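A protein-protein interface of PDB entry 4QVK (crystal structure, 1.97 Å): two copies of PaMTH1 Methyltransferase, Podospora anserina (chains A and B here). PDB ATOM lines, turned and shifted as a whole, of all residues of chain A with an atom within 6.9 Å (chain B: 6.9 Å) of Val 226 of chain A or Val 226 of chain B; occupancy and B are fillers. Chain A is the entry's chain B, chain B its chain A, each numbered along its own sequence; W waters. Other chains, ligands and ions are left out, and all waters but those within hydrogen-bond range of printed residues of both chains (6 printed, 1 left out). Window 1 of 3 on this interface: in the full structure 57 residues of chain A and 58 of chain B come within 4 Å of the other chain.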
ATOM      1  N   SER A   6      22.505   5.414 -22.666  1.00  0.00           N
ATOM      2  CA  SER A   6      21.963   6.766 -22.612  1.00  0.00           C
ATOM      3  C   SER A   6      20.449   6.837 -22.509  1.00  0.00           C
ATOM      4  O   SER A   6      19.863   7.894 -22.741  1.00  0.00           O
ATOM      5  CB  SER A   6      22.368   7.534 -23.869  1.00  0.00           C
ATOM      6  OG  SER A   6      23.701   7.252 -24.211  1.00  0.00           O
ATOM      7  N   ILE A   7      19.817   5.710 -22.226  1.00  0.00           N
ATOM      8  CA  ILE A   7      18.372   5.627 -22.234  1.00  0.00           C
ATOM      9  C   ILE A   7      17.884   5.082 -20.904  1.00  0.00           C
ATOM     10  O   ILE A   7      18.292   4.020 -20.485  1.00  0.00           O
ATOM     11  CB  ILE A   7      17.887   4.728 -23.394  1.00  0.00           C
ATOM     12  CG1 ILE A   7      18.344   5.357 -24.717  1.00  0.00           C
ATOM     13  CG2 ILE A   7      16.320   4.599 -23.376  1.00  0.00           C
ATOM     14  CD1 ILE A   7      18.047   4.495 -26.024  1.00  0.00           C
ATOM     15  N   LEU A   8      17.015   5.831 -20.250  1.00  0.00           N
ATOM     16  CA  LEU A   8      16.394   5.395 -19.009  1.00  0.00           C
ATOM     17  C   LEU A   8      15.330   4.350 -19.303  1.00  0.00           C
ATOM     18  O   LEU A   8      14.521   4.542 -20.220  1.00  0.00           O
ATOM     19  CB  LEU A   8      15.748   6.554 -18.279  1.00  0.00           C
ATOM     20  CG  LEU A   8      16.661   7.720 -17.883  1.00  0.00           C
ATOM     21  CD1 LEU A   8      15.785   8.735 -17.073  1.00  0.00           C
ATOM     22  CD2 LEU A   8      17.813   7.186 -17.024  1.00  0.00           C
ATOM     23  N   CYS A  22       6.816  15.942 -18.570  1.00  0.00           N
ATOM     24  CA  CYS A  22       7.445  16.841 -19.524  1.00  0.00           C
ATOM     25  C   CYS A  22       6.450  17.900 -20.059  1.00  0.00           C
ATOM     26  O   CYS A  22       6.780  19.103 -20.101  1.00  0.00           O
ATOM     27  CB  CYS A  22       8.067  16.048 -20.667  1.00  0.00           C
ATOM     28  SG  CYS A  22       9.469  14.989 -20.125  1.00  0.00           S
ATOM     29  N   GLN A  55       5.478  16.850 -28.490  1.00  0.00           N
ATOM     30  CA  GLN A  55       6.175  16.914 -29.763  1.00  0.00           C
ATOM     31  C   GLN A  55       5.823  18.214 -30.461  1.00  0.00           C
ATOM     32  O   GLN A  55       6.669  18.835 -31.090  1.00  0.00           O
ATOM     33  CB  GLN A  55       5.838  15.700 -30.639  1.00  0.00           C
ATOM     34  CG  GLN A  55       6.577  14.449 -30.127  1.00  0.00           C
ATOM     35  CD  GLN A  55       6.016  13.132 -30.660  1.00  0.00           C
ATOM     36  OE1 GLN A  55       4.969  12.649 -30.205  1.00  0.00           O
ATOM     37  NE2 GLN A  55       6.719  12.543 -31.611  1.00  0.00           N
ATOM     38  N   TRP A  58       7.881  20.733 -28.942  1.00  0.00           N
ATOM     39  CA  TRP A  58       9.258  20.554 -29.397  1.00  0.00           C
ATOM     40  C   TRP A  58       9.457  21.208 -30.780  1.00  0.00           C
ATOM     41  O   TRP A  58      10.450  21.939 -31.014  1.00  0.00           O
ATOM     42  CB  TRP A  58       9.597  19.064 -29.445  1.00  0.00           C
ATOM     43  CG  TRP A  58      10.876  18.724 -30.167  1.00  0.00           C
ATOM     44  CD1 TRP A  58      12.153  19.024 -29.776  1.00  0.00           C
ATOM     45  CD2 TRP A  58      10.992  18.008 -31.399  1.00  0.00           C
ATOM     46  NE1 TRP A  58      13.052  18.537 -30.698  1.00  0.00           N
ATOM     47  CE2 TRP A  58      12.363  17.906 -31.700  1.00  0.00           C
ATOM     48  CE3 TRP A  58      10.066  17.458 -32.278  1.00  0.00           C
ATOM     49  CZ2 TRP A  58      12.843  17.265 -32.849  1.00  0.00           C
ATOM     50  CZ3 TRP A  58      10.547  16.794 -33.429  1.00  0.00           C
ATOM     51  CH2 TRP A  58      11.921  16.705 -33.692  1.00  0.00           C
ATOM     52  N   ASP A 174      11.871  11.529 -38.371  1.00  0.00           N
ATOM     53  CA  ASP A 174      11.099  11.098 -37.206  1.00  0.00           C
ATOM     54  C   ASP A 174      10.746   9.594 -37.259  1.00  0.00           C
ATOM     55  O   ASP A 174      10.723   8.988 -38.329  1.00  0.00           O
ATOM     56  CB  ASP A 174       9.829  11.940 -37.097  1.00  0.00           C
ATOM     57  CG  ASP A 174       9.419  12.189 -35.664  1.00  0.00           C
ATOM     58  OD1 ASP A 174      10.200  11.902 -34.739  1.00  0.00           O
ATOM     59  OD2 ASP A 174       8.316  12.697 -35.451  1.00  0.00           O
ATOM     60  N   ASN A 175      10.467   9.007 -36.099  1.00  0.00           N
ATOM     61  CA  ASN A 175       9.999   7.609 -36.017  1.00  0.00           C
ATOM     62  C   ASN A 175      11.002   6.560 -36.476  1.00  0.00           C
ATOM     63  O   ASN A 175      10.642   5.447 -36.859  1.00  0.00           O
ATOM     64  CB  ASN A 175       8.697   7.435 -36.810  1.00  0.00           C
ATOM     65  CG  ASN A 175       7.501   8.040 -36.092  1.00  0.00           C
ATOM     66  OD1 ASN A 175       6.893   8.997 -36.590  1.00  0.00           O
ATOM     67  ND2 ASN A 175       7.152   7.501 -34.935  1.00  0.00           N
ATOM     68  N   PHE A 177      12.895   4.723 -34.906  1.00  0.00           N
ATOM     69  CA  PHE A 177      12.974   3.506 -34.067  1.00  0.00           C
ATOM     70  C   PHE A 177      11.900   2.462 -34.394  1.00  0.00           C
ATOM     71  O   PHE A 177      11.999   1.309 -33.974  1.00  0.00           O
ATOM     72  CB  PHE A 177      12.827   3.841 -32.578  1.00  0.00           C
ATOM     73  CG  PHE A 177      14.053   4.434 -31.934  1.00  0.00           C
ATOM     74  CD1 PHE A 177      15.281   4.452 -32.570  1.00  0.00           C
ATOM     75  CD2 PHE A 177      13.954   4.965 -30.653  1.00  0.00           C
ATOM     76  CE1 PHE A 177      16.422   5.013 -31.919  1.00  0.00           C
ATOM     77  CE2 PHE A 177      15.043   5.505 -30.010  1.00  0.00           C
ATOM     78  CZ  PHE A 177      16.301   5.526 -30.640  1.00  0.00           C
ATOM     79  N   LEU A 223      21.716   9.805 -34.337  1.00  0.00           N
ATOM     80  CA  LEU A 223      20.417   9.199 -34.032  1.00  0.00           C
ATOM     81  C   LEU A 223      20.103   9.444 -32.548  1.00  0.00           C
ATOM     82  O   LEU A 223      20.718   8.837 -31.637  1.00  0.00           O
ATOM     83  CB  LEU A 223      20.412   7.700 -34.359  1.00  0.00           C
ATOM     84  CG  LEU A 223      19.150   6.915 -34.016  1.00  0.00           C
ATOM     85  CD1 LEU A 223      17.895   7.664 -34.513  1.00  0.00           C
ATOM     86  CD2 LEU A 223      19.264   5.510 -34.638  1.00  0.00           C
ATOM     87  N   LEU A 224      19.188  10.366 -32.310  1.00  0.00           N
ATOM     88  CA  LEU A 224      18.871  10.785 -30.938  1.00  0.00           C
ATOM     89  C   LEU A 224      17.741   9.941 -30.328  1.00  0.00           C
ATOM     90  O   LEU A 224      16.668   9.877 -30.905  1.00  0.00           O
ATOM     91  CB  LEU A 224      18.487  12.260 -30.974  1.00  0.00           C
ATOM     92  CG  LEU A 224      18.452  13.171 -29.762  1.00  0.00           C
ATOM     93  CD1 LEU A 224      19.833  13.263 -29.204  1.00  0.00           C
ATOM     94  CD2 LEU A 224      17.949  14.547 -30.224  1.00  0.00           C
ATOM     95  N   PRO A 225      17.976   9.302 -29.152  1.00  0.00           N
ATOM     96  CA  PRO A 225      16.966   8.423 -28.559  1.00  0.00           C
ATOM     97  C   PRO A 225      15.845   9.195 -27.838  1.00  0.00           C
ATOM     98  O   PRO A 225      15.675   9.067 -26.620  1.00  0.00           O
ATOM     99  CB  PRO A 225      17.785   7.588 -27.555  1.00  0.00           C
ATOM    100  CG  PRO A 225      18.867   8.483 -27.137  1.00  0.00           C
ATOM    101  CD  PRO A 225      19.216   9.329 -28.341  1.00  0.00           C
ATOM    102  N   VAL A 226      15.092   9.991 -28.592  1.00  0.00           N
ATOM    103  CA  VAL A 226      14.023  10.813 -28.020  1.00  0.00           C
ATOM    104  C   VAL A 226      12.771  10.499 -28.826  1.00  0.00           C
ATOM    105  O   VAL A 226      12.898  10.144 -30.009  1.00  0.00           O
ATOM    106  CB  VAL A 226      14.353  12.321 -28.090  1.00  0.00           C
ATOM    107  CG1 VAL A 226      14.423  12.808 -29.579  1.00  0.00           C
ATOM    108  CG2 VAL A 226      13.296  13.107 -27.323  1.00  0.00           C
ATOM    109  N   PHE A 227      11.586  10.580 -28.206  1.00  0.00           N
ATOM    110  CA  PHE A 227      10.296  10.222 -28.852  1.00  0.00           C
ATOM    111  C   PHE A 227      10.388   8.810 -29.498  1.00  0.00           C
ATOM    112  O   PHE A 227      10.800   7.873 -28.840  1.00  0.00           O
ATOM    113  CB  PHE A 227       9.881  11.293 -29.865  1.00  0.00           C
ATOM    114  CG  PHE A 227       9.824  12.700 -29.280  1.00  0.00           C
ATOM    115  CD1 PHE A 227       9.152  12.950 -28.092  1.00  0.00           C
ATOM    116  CD2 PHE A 227      10.494  13.756 -29.888  1.00  0.00           C
ATOM    117  CE1 PHE A 227       9.095  14.284 -27.540  1.00  0.00           C
ATOM    118  CE2 PHE A 227      10.484  15.034 -29.339  1.00  0.00           C
ATOM    119  CZ  PHE A 227       9.766  15.310 -28.181  1.00  0.00           C
ATOM    120  N   ASP A 228      10.073   8.674 -30.780  1.00  0.00           N
ATOM    121  CA  ASP A 228      10.202   7.381 -31.455  1.00  0.00           C
ATOM    122  C   ASP A 228      11.467   7.283 -32.289  1.00  0.00           C
ATOM    123  O   ASP A 228      11.508   6.554 -33.283  1.00  0.00           O
ATOM    124  CB  ASP A 228       8.986   7.142 -32.356  1.00  0.00           C
ATOM    125  CG  ASP A 228       8.833   5.690 -32.812  1.00  0.00           C
ATOM    126  OD1 ASP A 228       9.354   4.765 -32.128  1.00  0.00           O
ATOM    127  OD2 ASP A 228       8.151   5.498 -33.869  1.00  0.00           O
ATOM    128  N   GLY A 229      12.510   7.994 -31.871  1.00  0.00           N
ATOM    129  CA  GLY A 229      13.793   7.940 -32.540  1.00  0.00           C
ATOM    130  C   GLY A 229      13.902   9.079 -33.529  1.00  0.00           C
ATOM    131  O   GLY A 229      13.133   9.111 -34.493  1.00  0.00           O
ATOM    132  N   VAL A 230      14.822  10.030 -33.306  1.00  0.00           N
ATOM    133  CA  VAL A 230      14.898  11.164 -34.234  1.00  0.00           C
ATOM    134  C   VAL A 230      16.287  11.244 -34.824  1.00  0.00           C
ATOM    135  O   VAL A 230      17.265  11.417 -34.076  1.00  0.00           O
ATOM    136  CB  VAL A 230      14.548  12.515 -33.533  1.00  0.00           C
ATOM    137  CG1 VAL A 230      14.828  13.741 -34.490  1.00  0.00           C
ATOM    138  CG2 VAL A 230      13.102  12.526 -33.083  1.00  0.00           C
ATOM    139  N   GLN A 232      19.075  13.273 -36.641  1.00  0.00           N
ATOM    140  CA  GLN A 232      19.576  14.567 -37.078  1.00  0.00           C
ATOM    141  C   GLN A 232      20.677  14.413 -38.153  1.00  0.00           C
ATOM    142  O   GLN A 232      21.641  13.648 -37.983  1.00  0.00           O
ATOM    143  CB  GLN A 232      20.118  15.340 -35.864  1.00  0.00           C
ATOM    144  CG  GLN A 232      19.065  15.492 -34.750  1.00  0.00           C
ATOM    145  CD  GLN A 232      19.582  16.323 -33.576  1.00  0.00           C
ATOM    146  OE1 GLN A 232      20.801  16.574 -33.415  1.00  0.00           O
ATOM    147  NE2 GLN A 232      18.679  16.768 -32.777  1.00  0.00           N
ATOM    148  N   SER B   6       5.151  10.347 -25.068  1.00  0.00           N
ATOM    149  CA  SER B   6       6.245  10.666 -25.969  1.00  0.00           C
ATOM    150  C   SER B   6       7.496   9.851 -25.666  1.00  0.00           C
ATOM    151  O   SER B   6       8.576  10.169 -26.155  1.00  0.00           O
ATOM    152  CB  SER B   6       6.596  12.149 -25.873  1.00  0.00           C
ATOM    153  OG  SER B   6       5.452  12.941 -26.085  1.00  0.00           O
ATOM    154  N   ILE B   7       7.356   8.833 -24.831  1.00  0.00           N
ATOM    155  CA  ILE B   7       8.509   8.040 -24.427  1.00  0.00           C
ATOM    156  C   ILE B   7       8.268   6.566 -24.720  1.00  0.00           C
ATOM    157  O   ILE B   7       7.256   6.029 -24.338  1.00  0.00           O
ATOM    158  CB  ILE B   7       8.797   8.257 -22.954  1.00  0.00           C
ATOM    159  CG1 ILE B   7       9.111   9.757 -22.712  1.00  0.00           C
ATOM    160  CG2 ILE B   7       9.900   7.276 -22.441  1.00  0.00           C
ATOM    161  CD1 ILE B   7       9.103  10.208 -21.226  1.00  0.00           C
ATOM    162  N   LEU B   8       9.199   5.912 -25.389  1.00  0.00           N
ATOM    163  CA  LEU B   8       9.091   4.468 -25.583  1.00  0.00           C
ATOM    164  C   LEU B   8       9.518   3.735 -24.308  1.00  0.00           C
ATOM    165  O   LEU B   8      10.566   4.025 -23.750  1.00  0.00           O
ATOM    166  CB  LEU B   8       9.965   4.011 -26.754  1.00  0.00           C
ATOM    167  CG  LEU B   8       9.574   4.538 -28.136  1.00  0.00           C
ATOM    168  CD1 LEU B   8      10.658   4.068 -29.126  1.00  0.00           C
ATOM    169  CD2 LEU B   8       8.166   4.069 -28.563  1.00  0.00           C
ATOM    170  N   CYS B  22      22.060   3.421 -31.312  1.00  0.00           N
ATOM    171  CA  CYS B  22      22.254   4.842 -31.608  1.00  0.00           C
ATOM    172  C   CYS B  22      23.721   5.178 -31.817  1.00  0.00           C
ATOM    173  O   CYS B  22      24.069   5.894 -32.787  1.00  0.00           O
ATOM    174  CB  CYS B  22      21.643   5.719 -30.491  1.00  0.00           C
ATOM    175  SG  CYS B  22      19.826   5.564 -30.380  1.00  0.00           S
ATOM    176  N   GLN B  55      26.285  10.678 -25.866  1.00  0.00           N
ATOM    177  CA  GLN B  55      26.049  12.032 -25.427  1.00  0.00           C
ATOM    178  C   GLN B  55      27.189  12.958 -25.864  1.00  0.00           C
ATOM    179  O   GLN B  55      26.976  14.130 -26.168  1.00  0.00           O
ATOM    180  CB  GLN B  55      25.849  12.062 -23.922  1.00  0.00           C
ATOM    181  CG  GLN B  55      25.037  13.269 -23.492  1.00  0.00           C
ATOM    182  CD  GLN B  55      24.248  13.017 -22.209  1.00  0.00           C
ATOM    183  OE1 GLN B  55      24.369  11.946 -21.571  1.00  0.00           O
ATOM    184  NE2 GLN B  55      23.434  14.028 -21.815  1.00  0.00           N
ATOM    185  N   TRP B  58      26.402  13.824 -29.310  1.00  0.00           N
ATOM    186  CA  TRP B  58      25.344  14.848 -29.299  1.00  0.00           C
ATOM    187  C   TRP B  58      25.895  16.227 -28.973  1.00  0.00           C
ATOM    188  O   TRP B  58      25.530  17.221 -29.612  1.00  0.00           O
ATOM    189  CB  TRP B  58      24.241  14.475 -28.303  1.00  0.00           C
ATOM    190  CG  TRP B  58      23.263  15.595 -27.942  1.00  0.00           C
ATOM    191  CD1 TRP B  58      22.271  16.123 -28.732  1.00  0.00           C
ATOM    192  CD2 TRP B  58      23.175  16.268 -26.686  1.00  0.00           C
ATOM    193  NE1 TRP B  58      21.588  17.105 -28.049  1.00  0.00           N
ATOM    194  CE2 TRP B  58      22.114  17.202 -26.782  1.00  0.00           C
ATOM    195  CE3 TRP B  58      23.888  16.164 -25.480  1.00  0.00           C
ATOM    196  CZ2 TRP B  58      21.761  18.051 -25.719  1.00  0.00           C
ATOM    197  CZ3 TRP B  58      23.540  16.992 -24.415  1.00  0.00           C
ATOM    198  CH2 TRP B  58      22.483  17.933 -24.544  1.00  0.00           C
ATOM    199  N   ASP B 174      21.278  19.410 -17.833  1.00  0.00           N
ATOM    200  CA  ASP B 174      21.365  17.953 -17.948  1.00  0.00           C
ATOM    201  C   ASP B 174      20.861  17.224 -16.687  1.00  0.00           C
ATOM    202  O   ASP B 174      20.777  17.820 -15.601  1.00  0.00           O
ATOM    203  CB  ASP B 174      22.822  17.551 -18.241  1.00  0.00           C
ATOM    204  CG  ASP B 174      22.924  16.320 -19.145  1.00  0.00           C
ATOM    205  OD1 ASP B 174      21.902  15.882 -19.677  1.00  0.00           O
ATOM    206  OD2 ASP B 174      24.031  15.788 -19.339  1.00  0.00           O
ATOM    207  N   ASN B 175      20.542  15.939 -16.855  1.00  0.00           N
ATOM    208  CA  ASN B 175      20.109  15.058 -15.766  1.00  0.00           C
ATOM    209  C   ASN B 175      18.911  15.554 -14.978  1.00  0.00           C
ATOM    210  O   ASN B 175      18.834  15.317 -13.776  1.00  0.00           O
ATOM    211  CB  ASN B 175      21.259  14.831 -14.760  1.00  0.00           C
ATOM    212  CG  ASN B 175      22.364  14.007 -15.333  1.00  0.00           C
ATOM    213  OD1 ASN B 175      23.457  14.522 -15.602  1.00  0.00           O
ATOM    214  ND2 ASN B 175      22.111  12.703 -15.505  1.00  0.00           N
ATOM    215  N   PHE B 177      15.874  14.558 -14.995  1.00  0.00           N
ATOM    216  CA  PHE B 177      14.972  13.499 -14.515  1.00  0.00           C
ATOM    217  C   PHE B 177      15.459  12.804 -13.214  1.00  0.00           C
ATOM    218  O   PHE B 177      14.688  12.096 -12.576  1.00  0.00           O
ATOM    219  CB  PHE B 177      14.774  12.390 -15.564  1.00  0.00           C
ATOM    220  CG  PHE B 177      13.903  12.768 -16.766  1.00  0.00           C
ATOM    221  CD1 PHE B 177      13.081  13.889 -16.774  1.00  0.00           C
ATOM    222  CD2 PHE B 177      13.918  11.939 -17.901  1.00  0.00           C
ATOM    223  CE1 PHE B 177      12.283  14.191 -17.923  1.00  0.00           C
ATOM    224  CE2 PHE B 177      13.145  12.238 -19.041  1.00  0.00           C
ATOM    225  CZ  PHE B 177      12.320  13.361 -19.038  1.00  0.00           C
ATOM    226  N   LEU B 223      11.154  20.623 -21.719  1.00  0.00           N
ATOM    227  CA  LEU B 223      11.813  19.519 -21.009  1.00  0.00           C
ATOM    228  C   LEU B 223      11.799  18.295 -21.919  1.00  0.00           C
ATOM    229  O   LEU B 223      10.748  17.679 -22.167  1.00  0.00           O
ATOM    230  CB  LEU B 223      11.148  19.230 -19.654  1.00  0.00           C
ATOM    231  CG  LEU B 223      11.662  17.997 -18.854  1.00  0.00           C
ATOM    232  CD1 LEU B 223      13.211  17.833 -18.763  1.00  0.00           C
ATOM    233  CD2 LEU B 223      11.073  18.025 -17.457  1.00  0.00           C
ATOM    234  N   LEU B 224      12.977  17.949 -22.426  1.00  0.00           N
ATOM    235  CA  LEU B 224      13.062  16.931 -23.445  1.00  0.00           C
ATOM    236  C   LEU B 224      13.415  15.574 -22.848  1.00  0.00           C
ATOM    237  O   LEU B 224      14.425  15.437 -22.126  1.00  0.00           O
ATOM    238  CB  LEU B 224      14.093  17.361 -24.485  1.00  0.00           C
ATOM    239  CG  LEU B 224      14.047  16.807 -25.901  1.00  0.00           C
ATOM    240  CD1 LEU B 224      12.799  17.280 -26.727  1.00  0.00           C
ATOM    241  CD2 LEU B 224      15.391  17.160 -26.572  1.00  0.00           C
ATOM    242  N   PRO B 225      12.601  14.555 -23.156  1.00  0.00           N
ATOM    243  CA  PRO B 225      12.824  13.243 -22.533  1.00  0.00           C
ATOM    244  C   PRO B 225      13.875  12.399 -23.279  1.00  0.00           C
ATOM    245  O   PRO B 225      13.605  11.305 -23.816  1.00  0.00           O
ATOM    246  CB  PRO B 225      11.423  12.598 -22.569  1.00  0.00           C
ATOM    247  CG  PRO B 225      10.758  13.197 -23.754  1.00  0.00           C
ATOM    248  CD  PRO B 225      11.309  14.609 -23.888  1.00  0.00           C
ATOM    249  N   VAL B 226      15.085  12.940 -23.305  1.00  0.00           N
ATOM    250  CA  VAL B 226      16.201  12.258 -23.921  1.00  0.00           C
ATOM    251  C   VAL B 226      17.254  12.136 -22.826  1.00  0.00           C
ATOM    252  O   VAL B 226      17.276  12.962 -21.918  1.00  0.00           O
ATOM    253  CB  VAL B 226      16.711  13.047 -25.157  1.00  0.00           C
ATOM    254  CG1 VAL B 226      17.245  14.426 -24.726  1.00  0.00           C
ATOM    255  CG2 VAL B 226      17.777  12.227 -25.975  1.00  0.00           C
ATOM    256  N   PHE B 227      18.081  11.096 -22.886  1.00  0.00           N
ATOM    257  CA  PHE B 227      19.181  10.872 -21.938  1.00  0.00           C
ATOM    258  C   PHE B 227      18.595  10.795 -20.537  1.00  0.00           C
ATOM    259  O   PHE B 227      17.668  10.041 -20.315  1.00  0.00           O
ATOM    260  CB  PHE B 227      20.265  11.948 -22.081  1.00  0.00           C
ATOM    261  CG  PHE B 227      20.859  12.011 -23.452  1.00  0.00           C
ATOM    262  CD1 PHE B 227      21.244  10.841 -24.101  1.00  0.00           C
ATOM    263  CD2 PHE B 227      21.015  13.223 -24.124  1.00  0.00           C
ATOM    264  CE1 PHE B 227      21.798  10.882 -25.400  1.00  0.00           C
ATOM    265  CE2 PHE B 227      21.580  13.282 -25.419  1.00  0.00           C
ATOM    266  CZ  PHE B 227      21.976  12.104 -26.062  1.00  0.00           C
ATOM    267  N   ASP B 228      19.128  11.545 -19.589  1.00  0.00           N
ATOM    268  CA  ASP B 228      18.555  11.589 -18.232  1.00  0.00           C
ATOM    269  C   ASP B 228      17.712  12.874 -18.052  1.00  0.00           C
ATOM    270  O   ASP B 228      17.605  13.418 -16.949  1.00  0.00           O
ATOM    271  CB  ASP B 228      19.682  11.517 -17.186  1.00  0.00           C
ATOM    272  CG  ASP B 228      19.170  11.267 -15.727  1.00  0.00           C
ATOM    273  OD1 ASP B 228      18.074  10.698 -15.528  1.00  0.00           O
ATOM    274  OD2 ASP B 228      19.921  11.624 -14.769  1.00  0.00           O
ATOM    275  N   GLY B 229      17.125  13.373 -19.143  1.00  0.00           N
ATOM    276  CA  GLY B 229      16.250  14.525 -19.054  1.00  0.00           C
ATOM    277  C   GLY B 229      17.022  15.797 -19.356  1.00  0.00           C
ATOM    278  O   GLY B 229      17.977  16.152 -18.640  1.00  0.00           O
ATOM    279  N   VAL B 230      16.654  16.484 -20.431  1.00  0.00           N
ATOM    280  CA  VAL B 230      17.354  17.717 -20.789  1.00  0.00           C
ATOM    281  C   VAL B 230      16.404  18.883 -20.862  1.00  0.00           C
ATOM    282  O   VAL B 230      15.490  18.878 -21.698  1.00  0.00           O
ATOM    283  CB  VAL B 230      18.062  17.575 -22.149  1.00  0.00           C
ATOM    284  CG1 VAL B 230      18.738  18.894 -22.512  1.00  0.00           C
ATOM    285  CG2 VAL B 230      19.085  16.408 -22.077  1.00  0.00           C
ATOM    286  N   GLN B 232      15.667  22.456 -22.132  1.00  0.00           N
ATOM    287  CA  GLN B 232      16.058  23.550 -23.015  1.00  0.00           C
ATOM    288  C   GLN B 232      15.382  24.850 -22.603  1.00  0.00           C
ATOM    289  O   GLN B 232      14.176  24.887 -22.357  1.00  0.00           O
ATOM    290  CB  GLN B 232      15.727  23.197 -24.480  1.00  0.00           C
ATOM    291  CG  GLN B 232      16.414  21.902 -24.964  1.00  0.00           C
ATOM    292  CD  GLN B 232      16.114  21.554 -26.433  1.00  0.00           C
ATOM    293  OE1 GLN B 232      15.197  22.090 -27.061  1.00  0.00           O
ATOM    294  NE2 GLN B 232      16.873  20.652 -26.966  1.00  0.00           N
HETATM  295  O   HOH W   1      11.426   7.486 -26.406  1.00  0.00           O
HETATM  296  O   HOH W   2      11.618  10.126 -25.416  1.00  0.00           O
HETATM  297  O   HOH W   3      16.161   8.286 -21.643  1.00  0.00           O
HETATM  298  O   HOH W   4      17.017   8.814 -24.339  1.00  0.00           O
HETATM  299  O   HOH W   5      12.071   3.433 -21.432  1.00  0.00           O
HETATM  300  O   HOH W   6      19.315  18.179 -29.997  1.00  0.00           O
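SG of Cys 22 of chain B lies close to O of Leu 223 of chain A, 3.6 Å away.
SG of Cys 22 of chain A lies close to O of Leu 223 of chain B.
ND2 of Asn 175 of chain B lies within hydrogen-bond range of OD2 of Asp 228 of chain B (2.5 Å).
O of Asp 228 of chain B lies within hydrogen-bond range of N of Phe 177 of chain B, 2.8 Å away.
OD2 of Asp 228 of chain A is in hydrogen-bond range of ND2 of Asn 175 of chain A (2.5 Å).
Among the printed residues, merely in contact across the chains: Ser 6 of chain A with Phe 227 of chain B (3.2 Å), Phe 227 of chain A with Ser 6 of chain B (3.2 Å), Asp 228 of chain A with Leu 8 of chain B (3.3 Å), Leu 8 of chain A with Asp 228 of chain B (3.4 Å), Cys 22 of chain A with Phe 177 of chain B (3.5 Å), Leu 8 of chain A with Phe 227 of chain B (3.5 Å), Phe 177 of chain A with Cys 22 of chain B (3.5 Å), Trp 58 of chain A with Leu 224 of chain B (3.6 Å), Phe 227 of chain A with Leu 8 of chain B (3.6 Å), Phe 177 of chain A with Leu 8 of chain B (3.7 Å), Leu 224 of chain A with Trp 58 of chain B (3.8 Å), Leu 8 of chain A with Phe 177 of chain B (3.8 Å), Val 226 of chain A with Val 226 of chain B (3.8 Å), Pro 225 of chain A with Val 226 of chain B (3.8 Å), Phe 227 of chain A with Leu 224 of chain B (3.9 Å), Cys 22 of chain A with Pro 225 of chain B (3.9 Å), Val 226 of chain A with Pro 225 of chain B (3.95 Å), Leu 224 of chain A with Val 226 of chain B (3.96 Å) and Leu 224 of chain A with Phe 227 of chain B (3.98 Å).
Val 226 of chain B touches just these residues of chain A: Leu 224, Pro 225 and Val 226.
Of the printed residues of chain B, Ser 6 of chain A touches Phe 227 (3.2 Å).
Of the printed residues of chain A, Pro 225 of chain B touches Cys 22 (3.9 Å) and Val 226 (3.95 Å).
Of the printed residues of chain A, Leu 224 of chain B touches Trp 58 and Phe 227.
Printed residues of chain B within 4 Å of Leu 224 of chain A: Trp 58 (3.8 Å), Val 226 (3.96 Å) and Phe 227 (3.98 Å).
The nearest residue of chain B that does not touch Val 226 of chain A is Leu 224 of chain B (4.03 Å).
The nearest residue of chain A that does not touch Val 226 of chain B is Ser 6 of chain A (5.0 Å).
The nearest printed residue of chain A that does not touch Pro 225 of chain B is Pro 225 of chain A (4.1 Å).
Of the 18 printed residues of chain A, 11 touch a printed residue of chain B.
Printed residues of chain A that touch a printed residue of chain B: Ser 6, Leu 8, Cys 22, Trp 58, Phe 177, Leu 223, Leu 224, Pro 225, Val 226, Phe 227 and Asp 228.
Hydrophobic or aromatic side chains of chain A that line the printed part of chain B: Leu 8, Trp 58, Phe 177, Leu 223, Leu 224, Val 226 and Phe 227.
Of the 18 printed residues of chain B, 11 touch a printed residue of chain A.
Among the printed residues, 21 pairs touch across the chains.
Among the printed residues, no Asp or Glu carboxylate lies within 4 Å of a Lys or Arg side-chain nitrogen of the other chain.
Cys 22 of chain A touches Leu 223 of chain B, and with the chains exchanged Leu 223 of chain A touches Cys 22 of chain B.
Leu 224 of chain A touches Val 226 of chain B, but with the chains exchanged Val 226 of chain A does not touch Leu 224 of chain B (4.03 Å).
Of the 21 pairs that touch across the chains among the printed residues, 19 have their exchanged pair printed and touching as well.
Water W1 bridges the backbone carbonyl oxygen (O) of Phe 227 of chain A (2.5 Å) and the backbone NH (N) of Leu 8 of chain B (2.9 Å).
Water W3 bridges the backbone carbonyl oxygen of Phe 227 of chain B (2.7 Å) and the backbone NH of Leu 8 of chain A (2.9 Å).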
